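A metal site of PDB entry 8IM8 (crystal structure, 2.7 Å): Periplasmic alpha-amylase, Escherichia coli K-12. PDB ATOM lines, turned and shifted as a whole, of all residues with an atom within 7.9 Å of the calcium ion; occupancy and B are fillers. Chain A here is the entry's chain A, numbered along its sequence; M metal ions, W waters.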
ATOM      1  N   THR A 196     -24.337  26.430 -17.692  1.00  0.00           N
ATOM      2  CA  THR A 196     -23.893  26.760 -16.355  1.00  0.00           C
ATOM      3  C   THR A 196     -24.910  26.346 -15.312  1.00  0.00           C
ATOM      4  O   THR A 196     -24.530  25.856 -14.241  1.00  0.00           O
ATOM      5  CB  THR A 196     -23.631  28.247 -16.247  1.00  0.00           C
ATOM      6  OG1 THR A 196     -22.726  28.585 -17.292  1.00  0.00           O
ATOM      7  CG2 THR A 196     -22.977  28.582 -14.906  1.00  0.00           C
ATOM      8  N   ASP A 197     -26.199  26.553 -15.590  1.00  0.00           N
ATOM      9  CA  ASP A 197     -27.206  26.206 -14.593  1.00  0.00           C
ATOM     10  C   ASP A 197     -27.210  24.710 -14.295  1.00  0.00           C
ATOM     11  O   ASP A 197     -27.731  24.288 -13.242  1.00  0.00           O
ATOM     12  CB  ASP A 197     -28.596  26.642 -15.033  1.00  0.00           C
ATOM     13  CG  ASP A 197     -29.623  26.423 -13.931  1.00  0.00           C
ATOM     14  OD1 ASP A 197     -29.655  27.201 -12.921  1.00  0.00           O
ATOM     15  OD2 ASP A 197     -30.371  25.423 -14.063  1.00  0.00           O
ATOM     16  N   GLU A 200     -22.684  23.409 -11.669  1.00  0.00           N
ATOM     17  CA  GLU A 200     -22.276  23.402 -10.277  1.00  0.00           C
ATOM     18  C   GLU A 200     -22.906  24.561  -9.518  1.00  0.00           C
ATOM     19  O   GLU A 200     -22.799  25.720  -9.942  1.00  0.00           O
ATOM     20  CB  GLU A 200     -20.760  23.474 -10.179  1.00  0.00           C
ATOM     21  CG  GLU A 200     -20.192  23.567  -8.766  1.00  0.00           C
ATOM     22  CD  GLU A 200     -20.579  22.391  -7.907  1.00  0.00           C
ATOM     23  OE1 GLU A 200     -20.983  21.362  -8.486  1.00  0.00           O
ATOM     24  OE2 GLU A 200     -20.444  22.491  -6.649  1.00  0.00           O
ATOM     25  N   ASN A 201     -23.559  24.266  -8.409  1.00  0.00           N
ATOM     26  CA  ASN A 201     -24.238  25.313  -7.673  1.00  0.00           C
ATOM     27  C   ASN A 201     -23.252  25.832  -6.632  1.00  0.00           C
ATOM     28  O   ASN A 201     -23.063  25.216  -5.573  1.00  0.00           O
ATOM     29  CB  ASN A 201     -25.531  24.810  -7.040  1.00  0.00           C
ATOM     30  CG  ASN A 201     -26.422  25.949  -6.557  1.00  0.00           C
ATOM     31  OD1 ASN A 201     -26.065  27.137  -6.705  1.00  0.00           O
ATOM     32  ND2 ASN A 201     -27.581  25.615  -6.002  1.00  0.00           N
ATOM     33  N   GLY A 202     -22.611  26.961  -6.944  1.00  0.00           N
ATOM     34  CA  GLY A 202     -21.675  27.564  -6.014  1.00  0.00           C
ATOM     35  C   GLY A 202     -22.319  28.409  -4.954  1.00  0.00           C
ATOM     36  O   GLY A 202     -21.727  28.610  -3.892  1.00  0.00           O
ATOM     37  N   ASP A 203     -23.523  28.877  -5.217  1.00  0.00           N
ATOM     38  CA  ASP A 203     -24.276  29.826  -4.410  1.00  0.00           C
ATOM     39  C   ASP A 203     -25.761  29.477  -4.503  1.00  0.00           C
ATOM     40  O   ASP A 203     -26.385  29.704  -5.554  1.00  0.00           O
ATOM     41  CB  ASP A 203     -24.021  31.267  -4.865  1.00  0.00           C
ATOM     42  CG  ASP A 203     -24.756  32.312  -4.007  1.00  0.00           C
ATOM     43  OD1 ASP A 203     -25.425  31.914  -3.015  1.00  0.00           O
ATOM     44  OD2 ASP A 203     -24.715  33.536  -4.333  1.00  0.00           O
ATOM     45  N   PRO A 204     -26.360  28.887  -3.465  1.00  0.00           N
ATOM     46  CA  PRO A 204     -27.786  28.563  -3.550  1.00  0.00           C
ATOM     47  C   PRO A 204     -28.706  29.701  -3.143  1.00  0.00           C
ATOM     48  O   PRO A 204     -29.931  29.578  -3.271  1.00  0.00           O
ATOM     49  CB  PRO A 204     -27.926  27.348  -2.607  1.00  0.00           C
ATOM     50  CG  PRO A 204     -26.823  27.472  -1.671  1.00  0.00           C
ATOM     51  CD  PRO A 204     -25.690  28.159  -2.376  1.00  0.00           C
ATOM     52  N   SER A 205     -28.153  30.830  -2.701  1.00  0.00           N
ATOM     53  CA  SER A 205     -28.983  31.976  -2.403  1.00  0.00           C
ATOM     54  C   SER A 205     -29.566  32.635  -3.646  1.00  0.00           C
ATOM     55  O   SER A 205     -30.439  33.493  -3.511  1.00  0.00           O
ATOM     56  CB  SER A 205     -28.182  33.020  -1.637  1.00  0.00           C
ATOM     57  OG  SER A 205     -27.210  33.618  -2.479  1.00  0.00           O
ATOM     58  N   ASN A 206     -29.074  32.286  -4.843  1.00  0.00           N
ATOM     59  CA  ASN A 206     -29.532  32.927  -6.075  1.00  0.00           C
ATOM     60  C   ASN A 206     -30.259  31.960  -6.983  1.00  0.00           C
ATOM     61  O   ASN A 206     -30.366  32.184  -8.199  1.00  0.00           O
ATOM     62  CB  ASN A 206     -28.353  33.580  -6.828  1.00  0.00           C
ATOM     63  CG  ASN A 206     -27.312  32.583  -7.309  1.00  0.00           C
ATOM     64  OD1 ASN A 206     -27.466  31.350  -7.186  1.00  0.00           O
ATOM     65  ND2 ASN A 206     -26.238  33.101  -7.865  1.00  0.00           N
ATOM     66  N   ASP A 207     -30.775  30.886  -6.416  1.00  0.00           N
ATOM     67  CA  ASP A 207     -31.318  29.850  -7.260  1.00  0.00           C
ATOM     68  C   ASP A 207     -32.707  30.192  -7.772  1.00  0.00           C
ATOM     69  O   ASP A 207     -33.080  29.736  -8.855  1.00  0.00           O
ATOM     70  CB  ASP A 207     -31.295  28.524  -6.510  1.00  0.00           C
ATOM     71  CG  ASP A 207     -29.874  27.994  -6.308  1.00  0.00           C
ATOM     72  OD1 ASP A 207     -28.977  28.310  -7.139  1.00  0.00           O
ATOM     73  OD2 ASP A 207     -29.664  27.252  -5.323  1.00  0.00           O
ATOM     74  N   GLN A 208     -33.470  31.011  -7.069  1.00  0.00           N
ATOM     75  CA  GLN A 208     -34.816  31.293  -7.513  1.00  0.00           C
ATOM     76  C   GLN A 208     -34.976  32.813  -7.654  1.00  0.00           C
ATOM     77  O   GLN A 208     -35.739  33.468  -6.940  1.00  0.00           O
ATOM     78  CB  GLN A 208     -35.893  30.659  -6.557  1.00  0.00           C
ATOM     79  CG  GLN A 208     -35.602  29.202  -6.135  1.00  0.00           C
ATOM     80  CD  GLN A 208     -35.386  29.080  -4.597  1.00  0.00           C
ATOM     81  OE1 GLN A 208     -36.039  29.820  -3.785  1.00  0.00           O
ATOM     82  NE2 GLN A 208     -34.466  28.183  -4.186  1.00  0.00           N
ATOM     83  N   SER A 209     -34.251  33.373  -8.595  1.00  0.00           N
ATOM     84  CA  SER A 209     -34.292  34.804  -8.794  1.00  0.00           C
ATOM     85  C   SER A 209     -35.584  35.195  -9.513  1.00  0.00           C
ATOM     86  O   SER A 209     -36.208  34.400 -10.217  1.00  0.00           O
ATOM     87  CB  SER A 209     -33.066  35.252  -9.590  1.00  0.00           C
ATOM     88  OG  SER A 209     -31.870  34.890  -8.892  1.00  0.00           O
ATOM     89  N   HIS A 224     -31.877  24.671 -12.245  1.00  0.00           N
ATOM     90  CA  HIS A 224     -31.425  23.819 -11.154  1.00  0.00           C
ATOM     91  C   HIS A 224     -30.510  24.548 -10.180  1.00  0.00           C
ATOM     92  O   HIS A 224     -30.404  24.095  -9.025  1.00  0.00           O
ATOM     93  CB  HIS A 224     -30.729  22.583 -11.709  1.00  0.00           C
ATOM     94  CG  HIS A 224     -31.621  21.738 -12.571  1.00  0.00           C
ATOM     95  ND1 HIS A 224     -31.187  20.601 -13.201  1.00  0.00           N
ATOM     96  CD2 HIS A 224     -32.912  21.899 -12.941  1.00  0.00           C
ATOM     97  CE1 HIS A 224     -32.175  20.076 -13.904  1.00  0.00           C
ATOM     98  NE2 HIS A 224     -33.233  20.851 -13.772  1.00  0.00           N
ATOM     99  N   GLY A 225     -29.870  25.645 -10.580  1.00  0.00           N
ATOM    100  CA  GLY A 225     -29.094  26.452  -9.654  1.00  0.00           C
ATOM    101  C   GLY A 225     -27.613  26.595  -9.994  1.00  0.00           C
ATOM    102  O   GLY A 225     -26.919  27.375  -9.311  1.00  0.00           O
ATOM    103  N   GLY A 226     -27.095  25.885 -10.999  1.00  0.00           N
ATOM    104  CA  GLY A 226     -25.697  26.041 -11.367  1.00  0.00           C
ATOM    105  C   GLY A 226     -25.455  27.508 -11.658  1.00  0.00           C
ATOM    106  O   GLY A 226     -26.390  28.182 -12.114  1.00  0.00           O
ATOM    107  N   ASP A 227     -24.263  28.013 -11.337  1.00  0.00           N
ATOM    108  CA  ASP A 227     -23.982  29.448 -11.378  1.00  0.00           C
ATOM    109  C   ASP A 227     -22.481  29.679 -11.597  1.00  0.00           C
ATOM    110  O   ASP A 227     -21.699  28.735 -11.774  1.00  0.00           O
ATOM    111  CB  ASP A 227     -24.550  30.120 -10.120  1.00  0.00           C
ATOM    112  CG  ASP A 227     -23.947  29.572  -8.824  1.00  0.00           C
ATOM    113  OD1 ASP A 227     -22.903  28.888  -8.858  1.00  0.00           O
ATOM    114  OD2 ASP A 227     -24.582  29.732  -7.762  1.00  0.00           O
ATOM    115  N   LEU A 228     -22.089  30.961 -11.668  1.00  0.00           N
ATOM    116  CA  LEU A 228     -20.707  31.293 -12.052  1.00  0.00           C
ATOM    117  C   LEU A 228     -19.717  30.937 -10.945  1.00  0.00           C
ATOM    118  O   LEU A 228     -18.620  30.470 -11.239  1.00  0.00           O
ATOM    119  CB  LEU A 228     -20.584  32.776 -12.423  1.00  0.00           C
ATOM    120  CG  LEU A 228     -21.290  33.237 -13.705  1.00  0.00           C
ATOM    121  CD1 LEU A 228     -21.228  34.720 -13.824  1.00  0.00           C
ATOM    122  CD2 LEU A 228     -20.678  32.572 -14.931  1.00  0.00           C
ATOM    123  N   ARG A 229     -20.090  31.119  -9.684  1.00  0.00           N
ATOM    124  CA  ARG A 229     -19.188  30.769  -8.601  1.00  0.00           C
ATOM    125  C   ARG A 229     -18.896  29.263  -8.598  1.00  0.00           C
ATOM    126  O   ARG A 229     -17.742  28.837  -8.418  1.00  0.00           O
ATOM    127  CB  ARG A 229     -19.771  31.270  -7.289  1.00  0.00           C
ATOM    128  CG  ARG A 229     -18.906  30.963  -6.102  1.00  0.00           C
ATOM    129  CD  ARG A 229     -19.533  31.533  -4.866  1.00  0.00           C
ATOM    130  NE  ARG A 229     -19.623  32.982  -4.974  1.00  0.00           N
ATOM    131  CZ  ARG A 229     -20.300  33.747  -4.125  1.00  0.00           C
ATOM    132  NH1 ARG A 229     -20.949  33.241  -3.091  1.00  0.00           N
ATOM    133  NH2 ARG A 229     -20.346  35.063  -4.334  1.00  0.00           N
ATOM    134  N   GLY A 230     -19.910  28.422  -8.836  1.00  0.00           N
ATOM    135  CA  GLY A 230     -19.653  26.986  -8.891  1.00  0.00           C
ATOM    136  C   GLY A 230     -18.726  26.612 -10.019  1.00  0.00           C
ATOM    137  O   GLY A 230     -17.764  25.830  -9.836  1.00  0.00           O
ATOM    138  N   ALA A 285     -29.553  37.215 -12.665  1.00  0.00           N
ATOM    139  CA  ALA A 285     -29.221  37.076 -11.244  1.00  0.00           C
ATOM    140  C   ALA A 285     -29.068  35.632 -10.804  1.00  0.00           C
ATOM    141  O   ALA A 285     -28.457  35.400  -9.756  1.00  0.00           O
ATOM    142  CB  ALA A 285     -30.269  37.757 -10.349  1.00  0.00           C
ATOM    143  N   ASN A 286     -29.599  34.653 -11.547  1.00  0.00           N
ATOM    144  CA  ASN A 286     -29.267  33.257 -11.267  1.00  0.00           C
ATOM    145  C   ASN A 286     -27.791  32.937 -11.469  1.00  0.00           C
ATOM    146  O   ASN A 286     -27.285  31.989 -10.858  1.00  0.00           O
ATOM    147  CB  ASN A 286     -30.126  32.298 -12.105  1.00  0.00           C
ATOM    148  CG  ASN A 286     -31.366  31.801 -11.344  1.00  0.00           C
ATOM    149  OD1 ASN A 286     -32.426  32.456 -11.335  1.00  0.00           O
ATOM    150  ND2 ASN A 286     -31.282  30.591 -10.811  1.00  0.00           N
ATOM    151  N   MET A 287     -27.082  33.727 -12.269  1.00  0.00           N
ATOM    152  CA  MET A 287     -25.700  33.431 -12.635  1.00  0.00           C
ATOM    153  C   MET A 287     -24.683  33.964 -11.623  1.00  0.00           C
ATOM    154  O   MET A 287     -23.591  33.388 -11.481  1.00  0.00           O
ATOM    155  CB  MET A 287     -25.437  34.000 -14.020  1.00  0.00           C
ATOM    156  CG  MET A 287     -26.155  33.263 -15.150  1.00  0.00           C
ATOM    157  SD  MET A 287     -25.478  31.611 -15.365  1.00  0.00           S
ATOM    158  CE  MET A 287     -26.841  30.593 -14.775  1.00  0.00           C
ATOM    159  N   GLY A 288     -25.039  35.029 -10.893  1.00  0.00           N
ATOM    160  CA  GLY A 288     -24.117  35.746 -10.039  1.00  0.00           C
ATOM    161  C   GLY A 288     -24.113  37.230 -10.387  1.00  0.00           C
ATOM    162  O   GLY A 288     -24.949  37.708 -11.168  1.00  0.00           O
HETATM  163 CA    CA M   1     -26.897  29.096  -7.514  1.00  0.00          CA
HETATM  164  O   HOH W   1     -27.966  30.097  -9.467  1.00  0.00           O
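N of Asp 227 lies within hydrogen-bond range of O of Glu 200.
The backbone NH (N) of Gly 225 sits at hydrogen-bond distance from the side-chain carboxylate (OD1) of Asp 197.
OD1 of Asp 227 lies within hydrogen-bond range of N of Gly 230, 3.0 Å away.
The side-chain carboxylate (OD1) of Asp 203 sits at hydrogen-bond distance from the side-chain hydroxyl (OG) of Ser 205, at 2.5 Å.
The backbone carbonyl oxygen (O) of Asn 206 sits at hydrogen-bond distance from the side-chain hydroxyl (OG) of Ser 209.
The side-chain carboxylate (OD2) of Asp 203 is in salt-bridge range of the guanidinium group (NH1) of Arg 229, at 3.98 Å.
The backbone carbonyl oxygen of Asn 206 is in hydrogen-bond range of the side-chain amide nitrogen of Asn 286 (3.2 Å).
The backbone carbonyl oxygen (O) of Asp 207 lies within hydrogen-bond range of the side-chain amide nitrogen (ND2) of Asn 286 (2.8 Å).
Water W1 bridges the backbone carbonyl oxygen (O) of Asn 286 and the backbone carbonyl oxygen (O) of Asn 206.
O of Asp 203 binds the calcium ion.
The calcium ion is bound by OD1 of Asp 207 (2.3 Å).
The calcium ion is bound by the side-chain amide oxygen (OD1) of Asn 201 (2.3 Å).
The calcium ion is bound by OD1 of Asn 206.
The side-chain carboxylate (OD2) of Asp 227 is bound to the calcium ion.
The calcium ion is bound by water W1 (2.4 Å).
The calcium ion is bound by the backbone carbonyl oxygen (O) of Gly 225, 2.5 Å away.
The calcium ion has seven donor atoms within binding distance.
Six residues have an atom within 4 Å of the calcium ion: Asn 201, Asp 203, Asn 206, Asp 207, Gly 225 and Asp 227.
Along chain A the residues within 4 Å of the calcium ion span positions 201 to 227.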
